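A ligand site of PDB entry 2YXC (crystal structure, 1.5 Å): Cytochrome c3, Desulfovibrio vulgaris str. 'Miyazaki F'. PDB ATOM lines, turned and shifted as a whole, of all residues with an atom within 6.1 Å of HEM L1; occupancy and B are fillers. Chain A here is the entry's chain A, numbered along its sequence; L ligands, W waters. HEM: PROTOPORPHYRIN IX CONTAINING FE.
SG of Cys 100 is covalently linked to CAB of HEM L1 (1.8 Å). CAC of HEM L1 is covalently linked to SG of Cys 105, at 1.8 Å. FE of HEM L1 is bound by NE2 of His 70, at 2.0 Å. A ring nitrogen (NE2) of His 106 binds an iron atom (FE) of HEM L1 (2.0 Å). O1D of HEM L1 lies within hydrogen-bond range of OH of Tyr 65 (2.6 Å). An oxygen (O2D) of HEM L1 lies within hydrogen-bond range of the backbone NH (N) of Thr 14. OG1 of Thr 14 is in hydrogen-bond range of O2D of HEM L1 (2.7 Å). N of Lys 13 is in hydrogen-bond range of O1D of HEM L1 (2.9 Å). N of Asp 12 is in hydrogen-bond range of O1D of HEM L1 (3.3 Å). A ring nitrogen (NE2) of His 83 is bound to an iron atom (FE) of HEM L2 (2.0 Å). A carbon (CAB) of HEM L2 is bonded to the side-chain sulfur of Cys 79, at 1.8 Å.
The backbone NH (N) of Cys 105 sits close to the side-chain hydroxyl (OG) of Ser 103 (3.2 Å). A ring nitrogen (ND1) of His 70 sits at hydrogen-bond distance from the backbone carbonyl oxygen (O) of Tyr 66, at 2.9 Å. The side-chain hydroxyl (OG) of Ser 103 sits at hydrogen-bond distance from the backbone NH (N) of His 106, at 3.1 Å. The backbone NH (N) of Met 11 sits at hydrogen-bond distance from the backbone carbonyl oxygen (O) of Val 18 (2.9 Å). O of Leu 97 sits at hydrogen-bond distance from ND1 of His 83 (2.9 Å). The side-chain hydroxyl (OG) of Ser 103 is in hydrogen-bond range of the backbone carbonyl oxygen (O) of Gly 99 (2.8 Å). O of Met 69 lies close to N of Cys 79 (3.3 Å). The backbone NH (N) of Val 80 is in hydrogen-bond range of the backbone carbonyl oxygen (O) of Met 69.
O2D of HEM L1 sits close to O of Met 11 (3.3 Å). Gln 16 touches HEM L1. CA of Pro 17 touches O2D of HEM L1 (3.6 Å). Val 18 touches HEM L1. Met 55 touches HEM L1 (O to O2A, 3.97 Å). NZ of Lys 57 touches CMA of HEM L1 (3.96 Å). CE2 of Tyr 66 touches C4A of HEM L1, at 3.4 Å. Met 69 touches HEM L1. Cys 79 touches HEM L1. CG2 of Val 80 touches C2C of HEM L1 (3.8 Å). His 83 touches HEM L1 (ND1 to CBC, 3.4 Å). O of Leu 97 touches CMC of HEM L1, 3.3 Å away. Thr 98 touches HEM L1. Gly 99 touches HEM L1 (O to CMC, 3.5 Å). Hydrophobic or aromatic side chains that line HEM L1: Met 11, Val 18, Tyr 65, Tyr 66, Met 69, His 70, Val 80, His 83 and His 106.
Water W4 lies within hydrogen-bond range of an oxygen (O1A) of HEM L1 and the backbone NH (N) of Lys 15. Water W6 bridges O2A of HEM L1 (2.6 Å) and O of Met 55 (2.7 Å). Water W3 bridges O1A of HEM L1 and NZ of Lys 57. Water W2 lies within hydrogen-bond range of an oxygen (O2A) of HEM L1 and the side-chain sulfur (SD) of Met 55. Water W1 lies within hydrogen-bond range of NE2 of Gln 16 (3.3 Å) and O1A of HEM L1 (3.4 Å).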
ATOM      1  N   MET A  11      29.390  -5.808  10.874  1.00  0.00           N
ATOM      2  CA  MET A  11      29.160  -7.136  11.420  1.00  0.00           C
ATOM      3  C   MET A  11      29.735  -8.122  10.410  1.00  0.00           C
ATOM      4  O   MET A  11      29.230  -8.242   9.299  1.00  0.00           O
ATOM      5  CB  MET A  11      27.659  -7.380  11.611  1.00  0.00           C
ATOM      6  CG  MET A  11      27.000  -6.334  12.507  1.00  0.00           C
ATOM      7  SD  MET A  11      25.230  -6.595  12.743  1.00  0.00           S
ATOM      8  CE  MET A  11      25.213  -8.044  13.798  1.00  0.00           C
ATOM      9  N   ASP A  12      30.819  -8.800  10.797  1.00  0.00           N
ATOM     10  CA  ASP A  12      31.577  -9.593   9.831  1.00  0.00           C
ATOM     11  C   ASP A  12      32.059 -10.933  10.379  1.00  0.00           C
ATOM     12  O   ASP A  12      33.175 -11.358  10.094  1.00  0.00           O
ATOM     13  CB  ASP A  12      32.766  -8.774   9.304  1.00  0.00           C
ATOM     14  CG  ASP A  12      33.606  -8.170  10.411  1.00  0.00           C
ATOM     15  OD1 ASP A  12      34.284  -7.149  10.150  1.00  0.00           O
ATOM     16  OD2 ASP A  12      33.610  -8.706  11.547  1.00  0.00           O
ATOM     17  N   LYS A  13      31.212 -11.612  11.145  1.00  0.00           N
ATOM     18  CA  LYS A  13      31.523 -12.950  11.626  1.00  0.00           C
ATOM     19  C   LYS A  13      31.434 -13.963  10.484  1.00  0.00           C
ATOM     20  O   LYS A  13      31.998 -15.057  10.572  1.00  0.00           O
ATOM     21  CB  LYS A  13      30.559 -13.370  12.735  1.00  0.00           C
ATOM     22  CG  LYS A  13      30.417 -12.366  13.870  1.00  0.00           C
ATOM     23  CD  LYS A  13      31.748 -12.007  14.506  1.00  0.00           C
ATOM     24  CE  LYS A  13      32.385 -13.212  15.187  1.00  0.00           C
ATOM     25  NZ  LYS A  13      33.605 -12.800  15.950  1.00  0.00           N
ATOM     26  N   THR A  14      30.738 -13.589   9.418  1.00  0.00           N
ATOM     27  CA  THR A  14      30.442 -14.532   8.332  1.00  0.00           C
ATOM     28  C   THR A  14      30.929 -14.009   6.982  1.00  0.00           C
ATOM     29  O   THR A  14      31.453 -12.893   6.887  1.00  0.00           O
ATOM     30  CB  THR A  14      28.930 -14.798   8.215  1.00  0.00           C
ATOM     31  OG1 THR A  14      28.288 -13.680   7.584  1.00  0.00           O
ATOM     32  CG2 THR A  14      28.323 -14.989   9.601  1.00  0.00           C
ATOM     33  N   LYS A  15      30.742 -14.811   5.942  1.00  0.00           N
ATOM     34  CA  LYS A  15      31.096 -14.402   4.587  1.00  0.00           C
ATOM     35  C   LYS A  15      30.002 -13.570   3.929  1.00  0.00           C
ATOM     36  O   LYS A  15      30.101 -13.197   2.755  1.00  0.00           O
ATOM     37  CB  LYS A  15      31.411 -15.631   3.724  1.00  0.00           C
ATOM     38  CG  LYS A  15      32.627 -16.411   4.193  1.00  0.00           C
ATOM     39  CD  LYS A  15      33.000 -17.509   3.215  1.00  0.00           C
ATOM     40  CE  LYS A  15      34.123 -18.380   3.774  1.00  0.00           C
ATOM     41  NZ  LYS A  15      34.535 -19.440   2.816  1.00  0.00           N
ATOM     42  N   GLN A  16      28.946 -13.266   4.683  1.00  0.00           N
ATOM     43  CA  GLN A  16      27.903 -12.349   4.215  1.00  0.00           C
ATOM     44  C   GLN A  16      27.825 -11.171   5.187  1.00  0.00           C
ATOM     45  O   GLN A  16      26.799 -10.960   5.832  1.00  0.00           O
ATOM     46  CB  GLN A  16      26.550 -13.070   4.169  1.00  0.00           C
ATOM     47  CG  GLN A  16      26.578 -14.440   3.497  1.00  0.00           C
ATOM     48  CD  GLN A  16      27.116 -14.390   2.083  1.00  0.00           C
ATOM     49  OE1 GLN A  16      26.868 -13.440   1.341  1.00  0.00           O
ATOM     50  NE2 GLN A  16      27.848 -15.431   1.697  1.00  0.00           N
ATOM     51  N   PRO A  17      28.904 -10.378   5.267  1.00  0.00           N
ATOM     52  CA  PRO A  17      28.955  -9.224   6.168  1.00  0.00           C
ATOM     53  C   PRO A  17      27.862  -8.179   5.943  1.00  0.00           C
ATOM     54  O   PRO A  17      27.434  -7.948   4.819  1.00  0.00           O
ATOM     55  CB  PRO A  17      30.354  -8.647   5.941  1.00  0.00           C
ATOM     56  CG  PRO A  17      30.724  -9.084   4.575  1.00  0.00           C
ATOM     57  CD  PRO A  17      30.086 -10.439   4.394  1.00  0.00           C
ATOM     58  N   VAL A  18      27.443  -7.558   7.036  1.00  0.00           N
ATOM     59  CA  VAL A  18      26.362  -6.580   7.007  1.00  0.00           C
ATOM     60  C   VAL A  18      26.776  -5.310   7.767  1.00  0.00           C
ATOM     61  O   VAL A  18      27.442  -5.390   8.800  1.00  0.00           O
ATOM     62  CB  VAL A  18      25.085  -7.155   7.657  1.00  0.00           C
ATOM     63  CG1 VAL A  18      24.002  -6.095   7.728  1.00  0.00           C
ATOM     64  CG2 VAL A  18      24.602  -8.353   6.850  1.00  0.00           C
ATOM     65  N   MET A  55      28.293 -20.703  15.086  1.00  0.00           N
ATOM     66  CA  MET A  55      28.256 -20.229  13.706  1.00  0.00           C
ATOM     67  C   MET A  55      27.683 -21.232  12.731  1.00  0.00           C
ATOM     68  O   MET A  55      27.838 -21.094  11.518  1.00  0.00           O
ATOM     69  CB  MET A  55      29.654 -19.808  13.267  1.00  0.00           C
ATOM     70  CG  MET A  55      30.157 -18.547  13.947  1.00  0.00           C
ATOM     71  SD  MET A  55      29.144 -17.093  13.544  1.00  0.00           S
ATOM     72  CE  MET A  55      29.374 -16.092  15.011  1.00  0.00           C
ATOM     73  N   ASP A  56      26.999 -22.244  13.250  1.00  0.00           N
ATOM     74  CA  ASP A  56      26.195 -23.097  12.380  1.00  0.00           C
ATOM     75  C   ASP A  56      24.842 -22.445  12.185  1.00  0.00           C
ATOM     76  O   ASP A  56      24.078 -22.272  13.136  1.00  0.00           O
ATOM     77  CB  ASP A  56      26.017 -24.489  12.999  1.00  0.00           C
ATOM     78  CG  ASP A  56      25.303 -25.442  12.054  1.00  0.00           C
ATOM     79  OD1 ASP A  56      24.097 -25.240  11.809  1.00  0.00           O
ATOM     80  OD2 ASP A  56      25.950 -26.385  11.557  1.00  0.00           O
ATOM     81  N   LYS A  57      24.548 -22.068  10.939  1.00  0.00           N
ATOM     82  CA  LYS A  57      23.369 -21.262  10.653  1.00  0.00           C
ATOM     83  C   LYS A  57      22.062 -22.036  10.779  1.00  0.00           C
ATOM     84  O   LYS A  57      20.984 -21.465  10.596  1.00  0.00           O
ATOM     85  CB  LYS A  57      23.479 -20.644   9.254  1.00  0.00           C
ATOM     86  CG  LYS A  57      23.523 -21.642   8.110  1.00  0.00           C
ATOM     87  CD  LYS A  57      23.647 -20.913   6.786  1.00  0.00           C
ATOM     88  CE  LYS A  57      23.706 -21.881   5.618  1.00  0.00           C
ATOM     89  NZ  LYS A  57      23.981 -21.162   4.340  1.00  0.00           N
ATOM     90  N   TYR A  65      24.067 -17.785  16.124  1.00  0.00           N
ATOM     91  CA  TYR A  65      24.274 -16.430  15.618  1.00  0.00           C
ATOM     92  C   TYR A  65      23.285 -16.088  14.499  1.00  0.00           C
ATOM     93  O   TYR A  65      22.631 -15.040  14.540  1.00  0.00           O
ATOM     94  CB  TYR A  65      25.710 -16.290  15.116  1.00  0.00           C
ATOM     95  CG  TYR A  65      26.077 -14.894  14.644  1.00  0.00           C
ATOM     96  CD1 TYR A  65      26.285 -14.635  13.296  1.00  0.00           C
ATOM     97  CD2 TYR A  65      26.246 -13.854  15.560  1.00  0.00           C
ATOM     98  CE1 TYR A  65      26.651 -13.362  12.854  1.00  0.00           C
ATOM     99  CE2 TYR A  65      26.619 -12.578  15.125  1.00  0.00           C
ATOM    100  CZ  TYR A  65      26.815 -12.338  13.780  1.00  0.00           C
ATOM    101  OH  TYR A  65      27.178 -11.089  13.336  1.00  0.00           O
ATOM    102  N   TYR A  66      23.176 -16.951  13.506  1.00  0.00           N
ATOM    103  CA  TYR A  66      22.245 -16.732  12.403  1.00  0.00           C
ATOM    104  C   TYR A  66      20.819 -16.601  12.928  1.00  0.00           C
ATOM    105  O   TYR A  66      20.066 -15.714  12.526  1.00  0.00           O
ATOM    106  CB  TYR A  66      22.316 -17.888  11.403  1.00  0.00           C
ATOM    107  CG  TYR A  66      21.375 -17.755  10.227  1.00  0.00           C
ATOM    108  CD1 TYR A  66      20.031 -18.133  10.332  1.00  0.00           C
ATOM    109  CD2 TYR A  66      21.811 -17.254   9.004  1.00  0.00           C
ATOM    110  CE1 TYR A  66      19.161 -18.003   9.261  1.00  0.00           C
ATOM    111  CE2 TYR A  66      20.951 -17.121   7.922  1.00  0.00           C
ATOM    112  CZ  TYR A  66      19.617 -17.495   8.058  1.00  0.00           C
ATOM    113  OH  TYR A  66      18.761 -17.361   7.001  1.00  0.00           O
ATOM    114  N   MET A  69      19.732 -13.268  14.291  1.00  0.00           N
ATOM    115  CA  MET A  69      19.594 -12.171  13.337  1.00  0.00           C
ATOM    116  C   MET A  69      18.408 -12.345  12.386  1.00  0.00           C
ATOM    117  O   MET A  69      17.915 -11.360  11.832  1.00  0.00           O
ATOM    118  CB  MET A  69      20.868 -12.014  12.512  1.00  0.00           C
ATOM    119  CG  MET A  69      22.135 -11.897  13.336  1.00  0.00           C
ATOM    120  SD  MET A  69      22.092 -10.535  14.520  1.00  0.00           S
ATOM    121  CE  MET A  69      23.551 -10.922  15.485  1.00  0.00           C
ATOM    122  N   HIS A  70      17.957 -13.580  12.185  1.00  0.00           N
ATOM    123  CA  HIS A  70      17.041 -13.864  11.092  1.00  0.00           C
ATOM    124  C   HIS A  70      15.657 -14.392  11.472  1.00  0.00           C
ATOM    125  O   HIS A  70      14.701 -14.197  10.726  1.00  0.00           O
ATOM    126  CB  HIS A  70      17.683 -14.862  10.109  1.00  0.00           C
ATOM    127  CG  HIS A  70      18.895 -14.336   9.410  1.00  0.00           C
ATOM    128  ND1 HIS A  70      20.169 -14.447   9.941  1.00  0.00           N
ATOM    129  CD2 HIS A  70      19.034 -13.726   8.214  1.00  0.00           C
ATOM    130  CE1 HIS A  70      21.039 -13.925   9.096  1.00  0.00           C
ATOM    131  NE2 HIS A  70      20.383 -13.474   8.035  1.00  0.00           N
ATOM    132  N   CYS A  79      16.718  -8.993  13.740  1.00  0.00           N
ATOM    133  CA  CYS A  79      16.776  -8.029  12.636  1.00  0.00           C
ATOM    134  C   CYS A  79      15.605  -8.235  11.697  1.00  0.00           C
ATOM    135  O   CYS A  79      14.829  -7.322  11.434  1.00  0.00           O
ATOM    136  CB  CYS A  79      18.058  -8.188  11.817  1.00  0.00           C
ATOM    137  SG  CYS A  79      19.620  -8.321  12.736  1.00  0.00           S
ATOM    138  N   VAL A  80      15.482  -9.455  11.184  1.00  0.00           N
ATOM    139  CA  VAL A  80      14.449  -9.743  10.201  1.00  0.00           C
ATOM    140  C   VAL A  80      13.060  -9.706  10.824  1.00  0.00           C
ATOM    141  O   VAL A  80      12.108  -9.222  10.213  1.00  0.00           O
ATOM    142  CB  VAL A  80      14.691 -11.119   9.544  1.00  0.00           C
ATOM    143  CG1 VAL A  80      13.549 -11.442   8.577  1.00  0.00           C
ATOM    144  CG2 VAL A  80      16.023 -11.115   8.804  1.00  0.00           C
ATOM    145  N   HIS A  83      11.976  -6.134  11.292  1.00  0.00           N
ATOM    146  CA  HIS A  83      11.814  -5.521   9.980  1.00  0.00           C
ATOM    147  C   HIS A  83      10.536  -6.003   9.296  1.00  0.00           C
ATOM    148  O   HIS A  83       9.905  -5.258   8.532  1.00  0.00           O
ATOM    149  CB  HIS A  83      13.019  -5.816   9.098  1.00  0.00           C
ATOM    150  CG  HIS A  83      14.228  -4.982   9.424  1.00  0.00           C
ATOM    151  ND1 HIS A  83      15.313  -4.900   8.577  1.00  0.00           N
ATOM    152  CD2 HIS A  83      14.516  -4.201  10.490  1.00  0.00           C
ATOM    153  CE1 HIS A  83      16.226  -4.112   9.112  1.00  0.00           C
ATOM    154  NE2 HIS A  83      15.770  -3.667  10.273  1.00  0.00           N
ATOM    155  N   GLU A  96      13.396  -4.455   0.646  1.00  0.00           N
ATOM    156  CA  GLU A  96      14.436  -3.609   1.211  1.00  0.00           C
ATOM    157  C   GLU A  96      14.920  -4.103   2.575  1.00  0.00           C
ATOM    158  O   GLU A  96      16.110  -4.083   2.870  1.00  0.00           O
ATOM    159  CB  GLU A  96      13.933  -2.168   1.382  1.00  0.00           C
ATOM    160  CG  GLU A  96      13.689  -1.420   0.086  1.00  0.00           C
ATOM    161  CD  GLU A  96      13.260   0.018   0.345  1.00  0.00           C
ATOM    162  OE1 GLU A  96      13.639   0.577   1.390  1.00  0.00           O
ATOM    163  OE2 GLU A  96      12.525   0.578  -0.496  1.00  0.00           O
ATOM    164  N   LEU A  97      13.973  -4.518   3.412  1.00  0.00           N
ATOM    165  CA  LEU A  97      14.284  -4.739   4.812  1.00  0.00           C
ATOM    166  C   LEU A  97      14.383  -6.207   5.227  1.00  0.00           C
ATOM    167  O   LEU A  97      14.978  -6.522   6.254  1.00  0.00           O
ATOM    168  CB  LEU A  97      13.250  -4.033   5.700  1.00  0.00           C
ATOM    169  CG  LEU A  97      13.116  -2.516   5.542  1.00  0.00           C
ATOM    170  CD1 LEU A  97      11.995  -2.027   6.446  1.00  0.00           C
ATOM    171  CD2 LEU A  97      14.430  -1.823   5.890  1.00  0.00           C
ATOM    172  N   THR A  98      13.817  -7.104   4.420  1.00  0.00           N
ATOM    173  CA  THR A  98      13.843  -8.523   4.787  1.00  0.00           C
ATOM    174  C   THR A  98      14.326  -9.453   3.674  1.00  0.00           C
ATOM    175  O   THR A  98      14.437 -10.653   3.883  1.00  0.00           O
ATOM    176  CB  THR A  98      12.453  -9.010   5.257  1.00  0.00           C
ATOM    177  OG1 THR A  98      11.543  -9.033   4.150  1.00  0.00           O
ATOM    178  CG2 THR A  98      11.904  -8.076   6.330  1.00  0.00           C
ATOM    179  N   GLY A  99      14.614  -8.891   2.497  1.00  0.00           N
ATOM    180  CA  GLY A  99      15.055  -9.715   1.386  1.00  0.00           C
ATOM    181  C   GLY A  99      16.389 -10.390   1.636  1.00  0.00           C
ATOM    182  O   GLY A  99      17.269  -9.815   2.278  1.00  0.00           O
ATOM    183  N   CYS A 100      16.556 -11.609   1.120  1.00  0.00           N
ATOM    184  CA  CYS A 100      17.778 -12.374   1.351  1.00  0.00           C
ATOM    185  C   CYS A 100      18.929 -11.915   0.450  1.00  0.00           C
ATOM    186  O   CYS A 100      20.095 -12.133   0.751  1.00  0.00           O
ATOM    187  CB  CYS A 100      17.522 -13.866   1.130  1.00  0.00           C
ATOM    188  SG  CYS A 100      16.190 -14.530   2.175  1.00  0.00           S
ATOM    189  N   LYS A 101      18.567 -11.293  -0.663  1.00  0.00           N
ATOM    190  CA  LYS A 101      19.540 -10.645  -1.536  1.00  0.00           C
ATOM    191  C   LYS A 101      18.903  -9.389  -2.108  1.00  0.00           C
ATOM    192  O   LYS A 101      17.675  -9.262  -2.121  1.00  0.00           O
ATOM    193  CB  LYS A 101      19.964 -11.591  -2.659  1.00  0.00           C
ATOM    194  CG  LYS A 101      18.841 -11.998  -3.600  1.00  0.00           C
ATOM    195  CD  LYS A 101      19.317 -13.023  -4.616  1.00  0.00           C
ATOM    196  CE  LYS A 101      18.411 -13.073  -5.830  1.00  0.00           C
ATOM    197  NZ  LYS A 101      18.493 -11.801  -6.614  1.00  0.00           N
ATOM    198  N   SER A 103      18.831  -6.610  -0.763  1.00  0.00           N
ATOM    199  CA  SER A 103      18.222  -5.860   0.333  1.00  0.00           C
ATOM    200  C   SER A 103      19.243  -4.916   0.938  1.00  0.00           C
ATOM    201  O   SER A 103      20.403  -4.880   0.532  1.00  0.00           O
ATOM    202  CB  SER A 103      17.693  -6.813   1.408  1.00  0.00           C
ATOM    203  OG  SER A 103      18.763  -7.442   2.101  1.00  0.00           O
ATOM    204  N   LYS A 104      18.812  -4.139   1.930  1.00  0.00           N
ATOM    205  CA  LYS A 104      19.708  -3.223   2.619  1.00  0.00           C
ATOM    206  C   LYS A 104      20.712  -3.958   3.511  1.00  0.00           C
ATOM    207  O   LYS A 104      21.718  -3.381   3.921  1.00  0.00           O
ATOM    208  CB  LYS A 104      18.904  -2.234   3.459  1.00  0.00           C
ATOM    209  CG  LYS A 104      18.113  -1.225   2.639  1.00  0.00           C
ATOM    210  CD  LYS A 104      19.020  -0.234   1.947  1.00  0.00           C
ATOM    211  CE  LYS A 104      18.245   0.959   1.413  1.00  0.00           C
ATOM    212  NZ  LYS A 104      17.235   0.552   0.396  1.00  0.00           N
ATOM    213  N   CYS A 105      20.449  -5.233   3.786  1.00  0.00           N
ATOM    214  CA  CYS A 105      21.394  -6.034   4.558  1.00  0.00           C
ATOM    215  C   CYS A 105      22.369  -6.795   3.675  1.00  0.00           C
ATOM    216  O   CYS A 105      23.575  -6.744   3.886  1.00  0.00           O
ATOM    217  CB  CYS A 105      20.646  -7.026   5.456  1.00  0.00           C
ATOM    218  SG  CYS A 105      19.582  -6.240   6.697  1.00  0.00           S
ATOM    219  N   HIS A 106      21.825  -7.511   2.697  1.00  0.00           N
ATOM    220  CA  HIS A 106      22.631  -8.323   1.778  1.00  0.00           C
ATOM    221  C   HIS A 106      22.459  -7.833   0.349  1.00  0.00           C
ATOM    222  O   HIS A 106      21.331  -7.741  -0.155  1.00  0.00           O
ATOM    223  CB  HIS A 106      22.200  -9.791   1.854  1.00  0.00           C
ATOM    224  CG  HIS A 106      22.369 -10.418   3.207  1.00  0.00           C
ATOM    225  ND1 HIS A 106      23.582 -10.479   3.862  1.00  0.00           N
ATOM    226  CD2 HIS A 106      21.479 -11.054   4.011  1.00  0.00           C
ATOM    227  CE1 HIS A 106      23.436 -11.144   5.000  1.00  0.00           C
ATOM    228  NE2 HIS A 106      22.166 -11.500   5.112  1.00  0.00           N
HETATM  229  CHA HEM L   1      24.354 -13.363   7.759  1.00  0.00           C
HETATM  230  CHB HEM L   1      21.181 -15.451   4.820  1.00  0.00           C
HETATM  231  CHC HEM L   1      18.255 -11.684   5.245  1.00  0.00           C
HETATM  232  CHD HEM L   1      21.267  -9.749   8.446  1.00  0.00           C
HETATM  233  C1A HEM L   1      23.825 -14.250   6.800  1.00  0.00           C
HETATM  234  C2A HEM L   1      24.413 -15.408   6.336  1.00  0.00           C
HETATM  235  C3A HEM L   1      23.536 -15.969   5.431  1.00  0.00           C
HETATM  236  C4A HEM L   1      22.401 -15.189   5.466  1.00  0.00           C
HETATM  237  CMA HEM L   1      23.752 -17.215   4.581  1.00  0.00           C
HETATM  238  CAA HEM L   1      25.749 -15.994   6.722  1.00  0.00           C
HETATM  239  CBA HEM L   1      25.601 -17.136   7.704  1.00  0.00           C
HETATM  240  CGA HEM L   1      26.893 -17.903   7.900  1.00  0.00           C
HETATM  241  O1A HEM L   1      27.451 -18.386   6.898  1.00  0.00           O
HETATM  242  O2A HEM L   1      27.349 -18.010   9.068  1.00  0.00           O
HETATM  243  C1B HEM L   1      20.001 -14.686   4.747  1.00  0.00           C
HETATM  244  C2B HEM L   1      18.818 -15.079   4.155  1.00  0.00           C
HETATM  245  C3B HEM L   1      17.963 -13.975   4.253  1.00  0.00           C
HETATM  246  C4B HEM L   1      18.676 -12.987   4.931  1.00  0.00           C
HETATM  247  CMB HEM L   1      18.557 -16.443   3.539  1.00  0.00           C
HETATM  248  CAB HEM L   1      16.644 -13.876   3.825  1.00  0.00           C
HETATM  249  CBB HEM L   1      15.625 -14.645   4.529  1.00  0.00           C
HETATM  250  C1C HEM L   1      18.873 -10.721   6.065  1.00  0.00           C
HETATM  251  C2C HEM L   1      18.404  -9.435   6.289  1.00  0.00           C
HETATM  252  C3C HEM L   1      19.257  -8.884   7.247  1.00  0.00           C
HETATM  253  C4C HEM L   1      20.212  -9.848   7.516  1.00  0.00           C
HETATM  254  CMC HEM L   1      17.218  -8.799   5.602  1.00  0.00           C
HETATM  255  CAC HEM L   1      19.178  -7.624   7.850  1.00  0.00           C
HETATM  256  CBC HEM L   1      17.892  -7.040   8.239  1.00  0.00           C
HETATM  257  C1D HEM L   1      22.347 -10.609   8.660  1.00  0.00           C
HETATM  258  C2D HEM L   1      23.361 -10.419   9.568  1.00  0.00           C
HETATM  259  C3D HEM L   1      24.298 -11.404   9.323  1.00  0.00           C
HETATM  260  C4D HEM L   1      23.757 -12.211   8.333  1.00  0.00           C
HETATM  261  CMD HEM L   1      23.441  -9.317  10.616  1.00  0.00           C
HETATM  262  CAD HEM L   1      25.651 -11.585   9.989  1.00  0.00           C
HETATM  263  CBD HEM L   1      26.732 -10.723   9.349  1.00  0.00           C
HETATM  264  CGD HEM L   1      28.120 -11.084   9.819  1.00  0.00           C
HETATM  265  O1D HEM L   1      28.392 -10.975  11.041  1.00  0.00           O
HETATM  266  O2D HEM L   1      28.951 -11.484   8.971  1.00  0.00           O
HETATM  267  NA  HEM L   1      22.641 -14.117   6.220  1.00  0.00           N
HETATM  268  NB  HEM L   1      19.871 -13.468   5.257  1.00  0.00           N
HETATM  269  NC  HEM L   1      19.996 -10.918   6.754  1.00  0.00           N
HETATM  270  ND  HEM L   1      22.563 -11.737   7.995  1.00  0.00           N
HETATM  271 FE   HEM L   1      21.277 -12.558   6.533  1.00  0.00          FE
HETATM  272  CHA HEM L   2      16.283  -0.046   9.143  1.00  0.00           C
HETATM  273  CHB HEM L   2      19.661  -3.437   9.619  1.00  0.00           C
HETATM  274  CHC HEM L   2      17.558  -4.881  13.701  1.00  0.00           C
HETATM  275  CHD HEM L   2      14.069  -1.633  13.097  1.00  0.00           C
HETATM  276  C1A HEM L   2      17.411  -0.833   8.889  1.00  0.00           C
HETATM  277  C2A HEM L   2      18.207  -0.724   7.766  1.00  0.00           C
HETATM  278  C3A HEM L   2      19.178  -1.717   7.888  1.00  0.00           C
HETATM  279  C4A HEM L   2      18.933  -2.362   9.083  1.00  0.00           C
HETATM  280  CMA HEM L   2      20.295  -2.031   6.897  1.00  0.00           C
HETATM  281  CAA HEM L   2      18.049   0.284   6.649  1.00  0.00           C
HETATM  282  CBA HEM L   2      18.657   1.631   6.989  1.00  0.00           C
HETATM  283  CGA HEM L   2      20.174   1.556   7.109  1.00  0.00           C
HETATM  284  O1A HEM L   2      20.835   1.420   6.057  1.00  0.00           O
HETATM  285  O2A HEM L   2      20.688   1.619   8.247  1.00  0.00           O
HETATM  286  C1B HEM L   2      19.418  -4.171  10.801  1.00  0.00           C
HETATM  287  C2B HEM L   2      20.163  -5.246  11.263  1.00  0.00           C
HETATM  288  C3B HEM L   2      19.577  -5.653  12.466  1.00  0.00           C
HETATM  289  C4B HEM L   2      18.474  -4.824  12.638  1.00  0.00           C
HETATM  290  CMB HEM L   2      21.357  -5.869  10.564  1.00  0.00           C
HETATM  291  CAB HEM L   2      19.978  -6.637  13.375  1.00  0.00           C
HETATM  292  CBB HEM L   2      21.388  -6.834  13.709  1.00  0.00           C
HETATM  293  C1C HEM L   2      16.383  -4.144  13.931  1.00  0.00           C
HETATM  294  C2C HEM L   2      15.495  -4.364  14.968  1.00  0.00           C
HETATM  295  C3C HEM L   2      14.450  -3.460  14.762  1.00  0.00           C
HETATM  296  C4C HEM L   2      14.800  -2.706  13.657  1.00  0.00           C
HETATM  297  CMC HEM L   2      15.716  -5.415  16.055  1.00  0.00           C
HETATM  298  CAC HEM L   2      13.268  -3.290  15.498  1.00  0.00           C
HETATM  299  CBC HEM L   2      13.074  -3.780  16.859  1.00  0.00           C
HETATM  300  C1D HEM L   2      14.355  -0.859  11.959  1.00  0.00           C
HETATM  301  C2D HEM L   2      13.565   0.168  11.457  1.00  0.00           C
HETATM  302  C3D HEM L   2      14.213   0.622  10.321  1.00  0.00           C
HETATM  303  C4D HEM L   2      15.356  -0.146  10.188  1.00  0.00           C
HETATM  304  CMD HEM L   2      12.259   0.672  12.048  1.00  0.00           C
HETATM  305  CAD HEM L   2      13.778   1.692   9.343  1.00  0.00           C
HETATM  306  CBD HEM L   2      12.778   1.167   8.329  1.00  0.00           C
HETATM  307  CGD HEM L   2      12.809   1.911   7.016  1.00  0.00           C
HETATM  308  O1D HEM L   2      11.837   1.789   6.243  1.00  0.00           O
HETATM  309  O2D HEM L   2      13.801   2.623   6.754  1.00  0.00           O
HETATM  310  NA  HEM L   2      17.867  -1.815   9.660  1.00  0.00           N
HETATM  311  NB  HEM L   2      18.403  -3.944  11.642  1.00  0.00           N
HETATM  312  NC  HEM L   2      15.966  -3.131  13.168  1.00  0.00           N
HETATM  313  ND  HEM L   2      15.431  -1.002  11.187  1.00  0.00           N
HETATM  314 FE   HEM L   2      16.906  -2.481  11.406  1.00  0.00          FE
HETATM  315  O   HOH W   1      28.451 -18.020   3.623  1.00  0.00           O
HETATM  316  O   HOH W   2      26.494 -17.642  11.550  1.00  0.00           O
HETATM  317  O   HOH W   3      26.471 -19.645   4.781  1.00  0.00           O
HETATM  318  O   HOH W   4      29.789 -17.584   6.093  1.00  0.00           O
HETATM  319  O   HOH W   5      21.463 -19.736   3.828  1.00  0.00           O
HETATM  320  O   HOH W   6      29.343 -19.386  10.025  1.00  0.00           O
